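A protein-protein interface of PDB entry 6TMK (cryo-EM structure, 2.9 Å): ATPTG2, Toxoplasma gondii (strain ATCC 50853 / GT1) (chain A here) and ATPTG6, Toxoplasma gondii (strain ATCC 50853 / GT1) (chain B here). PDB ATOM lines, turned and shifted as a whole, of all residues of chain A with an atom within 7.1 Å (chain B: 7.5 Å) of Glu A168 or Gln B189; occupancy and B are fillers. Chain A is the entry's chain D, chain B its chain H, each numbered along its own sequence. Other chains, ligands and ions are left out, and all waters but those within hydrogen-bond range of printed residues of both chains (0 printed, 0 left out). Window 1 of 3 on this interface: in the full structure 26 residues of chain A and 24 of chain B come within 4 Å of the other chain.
Along chain A the printed residues that touch a printed residue of chain B span positions 167 to 242. Of the 20 printed residues of chain B, 7 touch a printed residue of chain A. Printed residues of chain B that touch a printed residue of chain A: Asn B61, Tyr B65, Asp B66, Val B73, Gln B189, Ala B192 and Thr B193. Hydrophobic or aromatic side chains of chain B that line the printed part of chain A: Tyr B65, Val B73 and Ala B192. Among the printed residues, 10 pairs touch across the chains.
OD1 of Asp B66 touches OG of Ser A167, 3.6 Å away. Gln A172 touches Val B73. Thr A237 touches Gln B189 (O to NE2, 3.6 Å). Ala B192 touches Trp A238 (CB to CZ3, 3.8 Å).
OE1 of Gln A171 sits close to OE2 of Glu A168, at 3.0 Å. OD1 of Asn A239 sits close to N of Ala A242 (3.2 Å). OE1 of Gln A171 is in hydrogen-bond range of OG1 of Thr A237 (2.8 Å). OG1 of Thr B193 sits at hydrogen-bond distance from O of Gln B189, 3.0 Å away. OG1 of Thr A237 is in hydrogen-bond range of NH2 of Arg A175 (2.9 Å). N of Ser A167 lies within hydrogen-bond range of OE1 of Glu A170, 2.9 Å away.
Printed residues of chain A within 4 Å of Gln B189: Glu A168, Thr A237 and Asn A239. Of the printed residues of chain A, Val B73 touches Gln A172 (3.99 Å). Of the printed residues of chain A, Tyr B65 touches Asn A241 (3.3 Å). Printed residues of chain A within 4 Å of Asn B61: Ser A169. Ser B63 touches none of the printed residues of chain A. Asp A166 touches none of the printed residues of chain B. The nearest residue of chain B that does not touch Glu A168 is Asp B66 (4.1 Å). The nearest printed residue of chain B that does not touch Trp A238 is Gln B189 (4.3 Å).
ND2 of Asn A241 lies within hydrogen-bond range of O of Tyr B65. OG1 of Thr B193 is in hydrogen-bond range of O of Ala A242 (2.9 Å). The side-chain carboxylate of Asp B66 sits at hydrogen-bond distance from the side-chain hydroxyl of Ser A169, 2.5 Å away. ND2 of Asn B61 lies within hydrogen-bond range of OG of Ser A169 (3.4 Å). The side-chain amide nitrogen of Gln B189 sits at hydrogen-bond distance from the side-chain amide oxygen of Asn A239. The side-chain carboxylate of Glu A168 lies within hydrogen-bond range of the side-chain amide nitrogen of Gln B189 (2.6 Å).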
ATOM      1  N   ASP A 166      26.993 -10.912   6.603  1.00  0.00           N
ATOM      2  CA  ASP A 166      26.653  -9.882   7.564  1.00  0.00           C
ATOM      3  C   ASP A 166      27.272 -10.192   8.924  1.00  0.00           C
ATOM      4  O   ASP A 166      27.673 -11.318   9.218  1.00  0.00           O
ATOM      5  CB  ASP A 166      25.137  -9.759   7.689  1.00  0.00           C
ATOM      6  CG  ASP A 166      24.511  -9.067   6.502  1.00  0.00           C
ATOM      7  OD1 ASP A 166      23.306  -8.745   6.569  1.00  0.00           O
ATOM      8  OD2 ASP A 166      25.222  -8.843   5.500  1.00  0.00           O
ATOM      9  N   SER A 167      27.331  -9.168   9.761  1.00  0.00           N
ATOM     10  CA  SER A 167      27.685  -9.300  11.165  1.00  0.00           C
ATOM     11  C   SER A 167      26.435  -9.373  12.034  1.00  0.00           C
ATOM     12  O   SER A 167      25.314  -9.113  11.589  1.00  0.00           O
ATOM     13  CB  SER A 167      28.574  -8.134  11.596  1.00  0.00           C
ATOM     14  OG  SER A 167      27.848  -6.923  11.653  1.00  0.00           O
ATOM     15  N   GLU A 168      26.642  -9.760  13.292  1.00  0.00           N
ATOM     16  CA  GLU A 168      25.511  -9.926  14.197  1.00  0.00           C
ATOM     17  C   GLU A 168      24.807  -8.605  14.464  1.00  0.00           C
ATOM     18  O   GLU A 168      23.584  -8.580  14.637  1.00  0.00           O
ATOM     19  CB  GLU A 168      25.972 -10.558  15.503  1.00  0.00           C
ATOM     20  CG  GLU A 168      24.852 -11.261  16.249  1.00  0.00           C
ATOM     21  CD  GLU A 168      24.383 -12.512  15.543  1.00  0.00           C
ATOM     22  OE1 GLU A 168      25.240 -13.347  15.187  1.00  0.00           O
ATOM     23  OE2 GLU A 168      23.160 -12.653  15.327  1.00  0.00           O
ATOM     24  N   SER A 169      25.551  -7.498  14.484  1.00  0.00           N
ATOM     25  CA  SER A 169      24.923  -6.190  14.605  1.00  0.00           C
ATOM     26  C   SER A 169      23.992  -5.925  13.429  1.00  0.00           C
ATOM     27  O   SER A 169      22.873  -5.437  13.609  1.00  0.00           O
ATOM     28  CB  SER A 169      25.993  -5.105  14.706  1.00  0.00           C
ATOM     29  OG  SER A 169      26.898  -5.383  15.749  1.00  0.00           O
ATOM     30  N   GLU A 170      24.443  -6.237  12.214  1.00  0.00           N
ATOM     31  CA  GLU A 170      23.625  -6.010  11.031  1.00  0.00           C
ATOM     32  C   GLU A 170      22.397  -6.914  11.027  1.00  0.00           C
ATOM     33  O   GLU A 170      21.298  -6.484  10.651  1.00  0.00           O
ATOM     34  CB  GLU A 170      24.481  -6.223   9.786  1.00  0.00           C
ATOM     35  CG  GLU A 170      25.429  -5.080   9.519  1.00  0.00           C
ATOM     36  CD  GLU A 170      26.548  -5.427   8.559  1.00  0.00           C
ATOM     37  OE1 GLU A 170      27.019  -6.585   8.575  1.00  0.00           O
ATOM     38  OE2 GLU A 170      26.970  -4.536   7.793  1.00  0.00           O
ATOM     39  N   GLN A 171      22.564  -8.170  11.444  1.00  0.00           N
ATOM     40  CA  GLN A 171      21.427  -9.080  11.544  1.00  0.00           C
ATOM     41  C   GLN A 171      20.400  -8.555  12.538  1.00  0.00           C
ATOM     42  O   GLN A 171      19.193  -8.533  12.259  1.00  0.00           O
ATOM     43  CB  GLN A 171      21.901 -10.475  11.945  1.00  0.00           C
ATOM     44  CG  GLN A 171      22.741 -11.180  10.913  1.00  0.00           C
ATOM     45  CD  GLN A 171      22.967 -12.634  11.244  1.00  0.00           C
ATOM     46  OE1 GLN A 171      22.856 -13.049  12.393  1.00  0.00           O
ATOM     47  NE2 GLN A 171      23.278 -13.421  10.231  1.00  0.00           N
ATOM     48  N   GLN A 172      20.867  -8.136  13.713  1.00  0.00           N
ATOM     49  CA  GLN A 172      19.977  -7.590  14.725  1.00  0.00           C
ATOM     50  C   GLN A 172      19.276  -6.336  14.226  1.00  0.00           C
ATOM     51  O   GLN A 172      18.099  -6.116  14.525  1.00  0.00           O
ATOM     52  CB  GLN A 172      20.779  -7.297  15.988  1.00  0.00           C
ATOM     53  CG  GLN A 172      19.955  -7.016  17.209  1.00  0.00           C
ATOM     54  CD  GLN A 172      19.348  -8.252  17.807  1.00  0.00           C
ATOM     55  OE1 GLN A 172      19.385  -9.328  17.219  1.00  0.00           O
ATOM     56  NE2 GLN A 172      18.772  -8.103  18.983  1.00  0.00           N
ATOM     57  N   GLU A 173      19.985  -5.495  13.475  1.00  0.00           N
ATOM     58  CA  GLU A 173      19.377  -4.274  12.966  1.00  0.00           C
ATOM     59  C   GLU A 173      18.288  -4.578  11.947  1.00  0.00           C
ATOM     60  O   GLU A 173      17.231  -3.940  11.956  1.00  0.00           O
ATOM     61  CB  GLU A 173      20.443  -3.376  12.358  1.00  0.00           C
ATOM     62  CG  GLU A 173      21.285  -2.668  13.389  1.00  0.00           C
ATOM     63  CD  GLU A 173      22.491  -1.971  12.788  1.00  0.00           C
ATOM     64  OE1 GLU A 173      22.610  -1.946  11.544  1.00  0.00           O
ATOM     65  OE2 GLU A 173      23.326  -1.455  13.560  1.00  0.00           O
ATOM     66  N   ALA A 174      18.524  -5.543  11.061  1.00  0.00           N
ATOM     67  CA  ALA A 174      17.484  -5.957  10.127  1.00  0.00           C
ATOM     68  C   ALA A 174      16.271  -6.507  10.863  1.00  0.00           C
ATOM     69  O   ALA A 174      15.117  -6.224  10.502  1.00  0.00           O
ATOM     70  CB  ALA A 174      18.055  -7.001   9.178  1.00  0.00           C
ATOM     71  N   ARG A 175      16.522  -7.287  11.907  1.00  0.00           N
ATOM     72  CA  ARG A 175      15.450  -7.849  12.712  1.00  0.00           C
ATOM     73  C   ARG A 175      14.612  -6.740  13.343  1.00  0.00           C
ATOM     74  O   ARG A 175      13.374  -6.761  13.294  1.00  0.00           O
ATOM     75  CB  ARG A 175      16.077  -8.753  13.761  1.00  0.00           C
ATOM     76  CG  ARG A 175      15.351  -9.995  14.083  1.00  0.00           C
ATOM     77  CD  ARG A 175      16.204 -10.818  14.995  1.00  0.00           C
ATOM     78  NE  ARG A 175      17.254 -11.506  14.263  1.00  0.00           N
ATOM     79  CZ  ARG A 175      18.517 -11.599  14.665  1.00  0.00           C
ATOM     80  NH1 ARG A 175      18.922 -11.049  15.793  1.00  0.00           N
ATOM     81  NH2 ARG A 175      19.389 -12.248  13.925  1.00  0.00           N
ATOM     82  N   VAL A 236      16.453 -18.213  14.327  1.00  0.00           N
ATOM     83  CA  VAL A 236      17.873 -18.071  14.600  1.00  0.00           C
ATOM     84  C   VAL A 236      18.590 -17.807  13.286  1.00  0.00           C
ATOM     85  O   VAL A 236      18.078 -18.089  12.201  1.00  0.00           O
ATOM     86  CB  VAL A 236      18.462 -19.311  15.302  1.00  0.00           C
ATOM     87  CG1 VAL A 236      17.950 -19.391  16.715  1.00  0.00           C
ATOM     88  CG2 VAL A 236      18.104 -20.562  14.556  1.00  0.00           C
ATOM     89  N   THR A 237      19.799 -17.268  13.399  1.00  0.00           N
ATOM     90  CA  THR A 237      20.612 -16.950  12.240  1.00  0.00           C
ATOM     91  C   THR A 237      22.052 -17.340  12.514  1.00  0.00           C
ATOM     92  O   THR A 237      22.518 -17.328  13.655  1.00  0.00           O
ATOM     93  CB  THR A 237      20.539 -15.465  11.871  1.00  0.00           C
ATOM     94  OG1 THR A 237      20.655 -14.666  13.055  1.00  0.00           O
ATOM     95  CG2 THR A 237      19.241 -15.148  11.149  1.00  0.00           C
ATOM     96  N   TRP A 238      22.747 -17.683  11.440  1.00  0.00           N
ATOM     97  CA  TRP A 238      24.146 -18.066  11.459  1.00  0.00           C
ATOM     98  C   TRP A 238      24.904 -17.187  10.484  1.00  0.00           C
ATOM     99  O   TRP A 238      24.377 -16.817   9.431  1.00  0.00           O
ATOM    100  CB  TRP A 238      24.299 -19.529  11.081  1.00  0.00           C
ATOM    101  CG  TRP A 238      25.679 -20.072  11.176  1.00  0.00           C
ATOM    102  CD1 TRP A 238      26.430 -20.551  10.157  1.00  0.00           C
ATOM    103  CD2 TRP A 238      26.467 -20.223  12.358  1.00  0.00           C
ATOM    104  NE1 TRP A 238      27.638 -20.983  10.619  1.00  0.00           N
ATOM    105  CE2 TRP A 238      27.688 -20.791  11.972  1.00  0.00           C
ATOM    106  CE3 TRP A 238      26.259 -19.928  13.705  1.00  0.00           C
ATOM    107  CZ2 TRP A 238      28.700 -21.069  12.880  1.00  0.00           C
ATOM    108  CZ3 TRP A 238      27.267 -20.207  14.602  1.00  0.00           C
ATOM    109  CH2 TRP A 238      28.468 -20.769  14.186  1.00  0.00           C
ATOM    110  N   ASN A 239      26.136 -16.844  10.836  1.00  0.00           N
ATOM    111  CA  ASN A 239      26.939 -15.947  10.032  1.00  0.00           C
ATOM    112  C   ASN A 239      28.351 -16.493   9.938  1.00  0.00           C
ATOM    113  O   ASN A 239      28.705 -17.491  10.570  1.00  0.00           O
ATOM    114  CB  ASN A 239      26.986 -14.541  10.626  1.00  0.00           C
ATOM    115  CG  ASN A 239      27.464 -14.544  12.041  1.00  0.00           C
ATOM    116  OD1 ASN A 239      27.709 -15.597  12.621  1.00  0.00           O
ATOM    117  ND2 ASN A 239      27.640 -13.374  12.599  1.00  0.00           N
ATOM    118  N   PHE A 240      29.166 -15.798   9.155  1.00  0.00           N
ATOM    119  CA  PHE A 240      30.534 -16.212   8.913  1.00  0.00           C
ATOM    120  C   PHE A 240      31.452 -15.839  10.067  1.00  0.00           C
ATOM    121  O   PHE A 240      32.432 -16.545  10.326  1.00  0.00           O
ATOM    122  CB  PHE A 240      31.014 -15.577   7.612  1.00  0.00           C
ATOM    123  CG  PHE A 240      32.475 -15.689   7.380  1.00  0.00           C
ATOM    124  CD1 PHE A 240      33.072 -16.912   7.186  1.00  0.00           C
ATOM    125  CD2 PHE A 240      33.252 -14.560   7.344  1.00  0.00           C
ATOM    126  CE1 PHE A 240      34.417 -16.998   6.971  1.00  0.00           C
ATOM    127  CE2 PHE A 240      34.594 -14.643   7.128  1.00  0.00           C
ATOM    128  CZ  PHE A 240      35.177 -15.862   6.942  1.00  0.00           C
ATOM    129  N   ASN A 241      31.151 -14.755  10.777  1.00  0.00           N
ATOM    130  CA  ASN A 241      31.991 -14.317  11.880  1.00  0.00           C
ATOM    131  C   ASN A 241      31.801 -15.148  13.133  1.00  0.00           C
ATOM    132  O   ASN A 241      32.561 -14.973  14.090  1.00  0.00           O
ATOM    133  CB  ASN A 241      31.723 -12.859  12.221  1.00  0.00           C
ATOM    134  CG  ASN A 241      32.299 -11.908  11.213  1.00  0.00           C
ATOM    135  OD1 ASN A 241      33.207 -12.245  10.457  1.00  0.00           O
ATOM    136  ND2 ASN A 241      31.788 -10.696  11.214  1.00  0.00           N
ATOM    137  N   ALA A 242      30.820 -16.041  13.153  1.00  0.00           N
ATOM    138  CA  ALA A 242      30.675 -16.957  14.267  1.00  0.00           C
ATOM    139  C   ALA A 242      31.547 -18.190  14.112  1.00  0.00           C
ATOM    140  O   ALA A 242      31.745 -18.917  15.089  1.00  0.00           O
ATOM    141  CB  ALA A 242      29.211 -17.359  14.412  1.00  0.00           C
ATOM    142  N   MET B  60      26.981  -7.747  24.778  1.00  0.00           N
ATOM    143  CA  MET B  60      27.777  -6.917  23.891  1.00  0.00           C
ATOM    144  C   MET B  60      28.129  -7.689  22.630  1.00  0.00           C
ATOM    145  O   MET B  60      28.018  -8.915  22.571  1.00  0.00           O
ATOM    146  CB  MET B  60      29.044  -6.452  24.600  1.00  0.00           C
ATOM    147  CG  MET B  60      29.976  -7.576  24.924  1.00  0.00           C
ATOM    148  SD  MET B  60      30.934  -7.243  26.401  1.00  0.00           S
ATOM    149  CE  MET B  60      32.245  -6.304  25.663  1.00  0.00           C
ATOM    150  N   ASN B  61      28.554  -6.944  21.615  1.00  0.00           N
ATOM    151  CA  ASN B  61      29.155  -7.541  20.432  1.00  0.00           C
ATOM    152  C   ASN B  61      30.637  -7.805  20.671  1.00  0.00           C
ATOM    153  O   ASN B  61      31.312  -7.064  21.388  1.00  0.00           O
ATOM    154  CB  ASN B  61      28.970  -6.637  19.216  1.00  0.00           C
ATOM    155  CG  ASN B  61      27.560  -6.092  19.096  1.00  0.00           C
ATOM    156  OD1 ASN B  61      27.322  -4.903  19.299  1.00  0.00           O
ATOM    157  ND2 ASN B  61      26.619  -6.959  18.767  1.00  0.00           N
ATOM    158  N   SER B  62      31.146  -8.862  20.044  1.00  0.00           N
ATOM    159  CA  SER B  62      32.471  -9.380  20.363  1.00  0.00           C
ATOM    160  C   SER B  62      33.459  -9.339  19.209  1.00  0.00           C
ATOM    161  O   SER B  62      34.643  -9.079  19.435  1.00  0.00           O
ATOM    162  CB  SER B  62      32.363 -10.825  20.859  1.00  0.00           C
ATOM    163  OG  SER B  62      31.892 -11.682  19.834  1.00  0.00           O
ATOM    164  N   SER B  63      33.024  -9.596  17.980  1.00  0.00           N
ATOM    165  CA  SER B  63      33.970  -9.793  16.894  1.00  0.00           C
ATOM    166  C   SER B  63      34.627  -8.483  16.480  1.00  0.00           C
ATOM    167  O   SER B  63      34.015  -7.414  16.513  1.00  0.00           O
ATOM    168  CB  SER B  63      33.269 -10.420  15.689  1.00  0.00           C
ATOM    169  OG  SER B  63      34.199 -10.775  14.686  1.00  0.00           O
ATOM    170  N   TYR B  65      35.546  -8.078  13.449  1.00  0.00           N
ATOM    171  CA  TYR B  65      34.940  -7.856  12.152  1.00  0.00           C
ATOM    172  C   TYR B  65      33.505  -7.381  12.263  1.00  0.00           C
ATOM    173  O   TYR B  65      32.734  -7.531  11.311  1.00  0.00           O
ATOM    174  CB  TYR B  65      35.023  -9.138  11.334  1.00  0.00           C
ATOM    175  CG  TYR B  65      36.427  -9.651  11.199  1.00  0.00           C
ATOM    176  CD1 TYR B  65      37.292  -9.111  10.270  1.00  0.00           C
ATOM    177  CD2 TYR B  65      36.899 -10.655  12.021  1.00  0.00           C
ATOM    178  CE1 TYR B  65      38.573  -9.572  10.149  1.00  0.00           C
ATOM    179  CE2 TYR B  65      38.175 -11.120  11.909  1.00  0.00           C
ATOM    180  CZ  TYR B  65      39.016 -10.572  10.974  1.00  0.00           C
ATOM    181  OH  TYR B  65      40.302 -11.035  10.856  1.00  0.00           O
ATOM    182  N   ASP B  66      33.139  -6.822  13.407  1.00  0.00           N
ATOM    183  CA  ASP B  66      31.907  -6.082  13.587  1.00  0.00           C
ATOM    184  C   ASP B  66      32.243  -4.625  13.847  1.00  0.00           C
ATOM    185  O   ASP B  66      33.226  -4.319  14.530  1.00  0.00           O
ATOM    186  CB  ASP B  66      31.091  -6.656  14.744  1.00  0.00           C
ATOM    187  CG  ASP B  66      29.667  -6.159  14.764  1.00  0.00           C
ATOM    188  OD1 ASP B  66      29.415  -5.049  14.257  1.00  0.00           O
ATOM    189  OD2 ASP B  66      28.795  -6.884  15.280  1.00  0.00           O
ATOM    190  N   VAL B  73      24.325  -4.729  22.863  1.00  0.00           N
ATOM    191  CA  VAL B  73      23.368  -5.208  21.881  1.00  0.00           C
ATOM    192  C   VAL B  73      22.105  -4.368  21.960  1.00  0.00           C
ATOM    193  O   VAL B  73      21.616  -4.035  23.047  1.00  0.00           O
ATOM    194  CB  VAL B  73      23.076  -6.701  22.088  1.00  0.00           C
ATOM    195  CG1 VAL B  73      21.963  -7.149  21.186  1.00  0.00           C
ATOM    196  CG2 VAL B  73      24.313  -7.510  21.799  1.00  0.00           C
ATOM    197  N   LYS B 137      16.219 -16.937  27.551  1.00  0.00           N
ATOM    198  CA  LYS B 137      17.435 -16.167  27.350  1.00  0.00           C
ATOM    199  C   LYS B 137      17.516 -14.950  28.257  1.00  0.00           C
ATOM    200  O   LYS B 137      18.605 -14.600  28.719  1.00  0.00           O
ATOM    201  CB  LYS B 137      17.501 -15.713  25.893  1.00  0.00           C
ATOM    202  CG  LYS B 137      18.769 -15.044  25.490  1.00  0.00           C
ATOM    203  CD  LYS B 137      18.763 -14.738  24.023  1.00  0.00           C
ATOM    204  CE  LYS B 137      19.852 -13.758  23.677  1.00  0.00           C
ATOM    205  NZ  LYS B 137      19.935 -13.501  22.227  1.00  0.00           N
ATOM    206  N   GLN B 183      26.973 -21.963  28.404  1.00  0.00           N
ATOM    207  CA  GLN B 183      25.774 -21.209  28.757  1.00  0.00           C
ATOM    208  C   GLN B 183      25.063 -20.706  27.504  1.00  0.00           C
ATOM    209  O   GLN B 183      24.818 -19.512  27.328  1.00  0.00           O
ATOM    210  CB  GLN B 183      26.122 -20.039  29.680  1.00  0.00           C
ATOM    211  CG  GLN B 183      26.824 -20.415  30.952  1.00  0.00           C
ATOM    212  CD  GLN B 183      25.926 -21.057  31.968  1.00  0.00           C
ATOM    213  OE1 GLN B 183      24.703 -21.013  31.859  1.00  0.00           O
ATOM    214  NE2 GLN B 183      26.530 -21.666  32.967  1.00  0.00           N
ATOM    215  N   ALA B 184      24.712 -21.650  26.636  1.00  0.00           N
ATOM    216  CA  ALA B 184      24.104 -21.280  25.370  1.00  0.00           C
ATOM    217  C   ALA B 184      22.680 -20.775  25.534  1.00  0.00           C
ATOM    218  O   ALA B 184      22.149 -20.156  24.607  1.00  0.00           O
ATOM    219  CB  ALA B 184      24.134 -22.475  24.421  1.00  0.00           C
ATOM    220  N   ILE B 186      21.823 -18.346  27.392  1.00  0.00           N
ATOM    221  CA  ILE B 186      21.938 -16.900  27.505  1.00  0.00           C
ATOM    222  C   ILE B 186      22.913 -16.303  26.496  1.00  0.00           C
ATOM    223  O   ILE B 186      22.803 -15.106  26.192  1.00  0.00           O
ATOM    224  CB  ILE B 186      22.317 -16.482  28.938  1.00  0.00           C
ATOM    225  CG1 ILE B 186      23.686 -17.026  29.322  1.00  0.00           C
ATOM    226  CG2 ILE B 186      21.291 -16.992  29.910  1.00  0.00           C
ATOM    227  CD1 ILE B 186      24.128 -16.604  30.678  1.00  0.00           C
ATOM    228  N   ASP B 187      23.864 -17.080  25.984  1.00  0.00           N
ATOM    229  CA  ASP B 187      24.796 -16.648  24.944  1.00  0.00           C
ATOM    230  C   ASP B 187      24.874 -17.730  23.878  1.00  0.00           C
ATOM    231  O   ASP B 187      25.896 -18.416  23.730  1.00  0.00           O
ATOM    232  CB  ASP B 187      26.179 -16.351  25.524  1.00  0.00           C
ATOM    233  CG  ASP B 187      26.209 -15.078  26.334  1.00  0.00           C
ATOM    234  OD1 ASP B 187      26.104 -15.160  27.573  1.00  0.00           O
ATOM    235  OD2 ASP B 187      26.341 -13.993  25.729  1.00  0.00           O
ATOM    236  N   PRO B 188      23.808 -17.892  23.093  1.00  0.00           N
ATOM    237  CA  PRO B 188      23.802 -18.979  22.104  1.00  0.00           C
ATOM    238  C   PRO B 188      24.815 -18.797  20.991  1.00  0.00           C
ATOM    239  O   PRO B 188      25.436 -19.777  20.571  1.00  0.00           O
ATOM    240  CB  PRO B 188      22.361 -18.958  21.571  1.00  0.00           C
ATOM    241  CG  PRO B 188      21.616 -17.971  22.407  1.00  0.00           C
ATOM    242  CD  PRO B 188      22.602 -17.060  23.006  1.00  0.00           C
ATOM    243  N   GLN B 189      24.997 -17.577  20.490  1.00  0.00           N
ATOM    244  CA  GLN B 189      25.955 -17.363  19.412  1.00  0.00           C
ATOM    245  C   GLN B 189      27.386 -17.597  19.888  1.00  0.00           C
ATOM    246  O   GLN B 189      28.174 -18.289  19.220  1.00  0.00           O
ATOM    247  CB  GLN B 189      25.787 -15.942  18.880  1.00  0.00           C
ATOM    248  CG  GLN B 189      26.247 -15.714  17.451  1.00  0.00           C
ATOM    249  CD  GLN B 189      25.310 -16.314  16.421  1.00  0.00           C
ATOM    250  OE1 GLN B 189      24.386 -17.052  16.757  1.00  0.00           O
ATOM    251  NE2 GLN B 189      25.528 -15.973  15.157  1.00  0.00           N
ATOM    252  N   GLY B 190      27.693 -17.135  21.101  1.00  0.00           N
ATOM    253  CA  GLY B 190      28.997 -17.391  21.674  1.00  0.00           C
ATOM    254  C   GLY B 190      29.238 -18.858  21.931  1.00  0.00           C
ATOM    255  O   GLY B 190      30.371 -19.328  21.822  1.00  0.00           O
ATOM    256  N   ALA B 191      28.186 -19.605  22.260  1.00  0.00           N
ATOM    257  CA  ALA B 191      28.399 -21.006  22.589  1.00  0.00           C
ATOM    258  C   ALA B 191      28.513 -21.828  21.312  1.00  0.00           C
ATOM    259  O   ALA B 191      29.305 -22.777  21.243  1.00  0.00           O
ATOM    260  CB  ALA B 191      27.269 -21.507  23.477  1.00  0.00           C
ATOM    261  N   ALA B 192      27.719 -21.481  20.299  1.00  0.00           N
ATOM    262  CA  ALA B 192      27.788 -22.188  19.031  1.00  0.00           C
ATOM    263  C   ALA B 192      29.173 -22.025  18.434  1.00  0.00           C
ATOM    264  O   ALA B 192      29.723 -22.958  17.832  1.00  0.00           O
ATOM    265  CB  ALA B 192      26.714 -21.659  18.088  1.00  0.00           C
ATOM    266  N   THR B 193      29.767 -20.847  18.638  1.00  0.00           N
ATOM    267  CA  THR B 193      31.133 -20.610  18.191  1.00  0.00           C
ATOM    268  C   THR B 193      32.113 -21.593  18.825  1.00  0.00           C
ATOM    269  O   THR B 193      33.143 -21.913  18.224  1.00  0.00           O
ATOM    270  CB  THR B 193      31.544 -19.177  18.519  1.00  0.00           C
ATOM    271  OG1 THR B 193      30.767 -18.261  17.744  1.00  0.00           O
ATOM    272  CG2 THR B 193      32.997 -18.958  18.219  1.00  0.00           C
ATOM    273  N   LYS B 194      31.819 -22.073  20.033  1.00  0.00           N
ATOM    274  CA  LYS B 194      32.658 -23.059  20.702  1.00  0.00           C
ATOM    275  C   LYS B 194      32.334 -24.494  20.313  1.00  0.00           C
ATOM    276  O   LYS B 194      33.226 -25.348  20.338  1.00  0.00           O
ATOM    277  CB  LYS B 194      32.511 -22.932  22.215  1.00  0.00           C
ATOM    278  CG  LYS B 194      32.526 -21.525  22.740  1.00  0.00           C
ATOM    279  CD  LYS B 194      33.828 -20.836  22.523  1.00  0.00           C
ATOM    280  CE  LYS B 194      34.046 -19.795  23.594  1.00  0.00           C
ATOM    281  NZ  LYS B 194      32.844 -18.949  23.792  1.00  0.00           N
ATOM    282  N   CYS B 195      31.082 -24.785  19.976  1.00  0.00           N
ATOM    283  CA  CYS B 195      30.612 -26.159  19.852  1.00  0.00           C
ATOM    284  C   CYS B 195      30.507 -26.642  18.408  1.00  0.00           C
ATOM    285  O   CYS B 195      30.285 -27.847  18.172  1.00  0.00           O
ATOM    286  CB  CYS B 195      29.261 -26.299  20.556  1.00  0.00           C
ATOM    287  SG  CYS B 195      29.368 -25.883  22.303  1.00  0.00           S
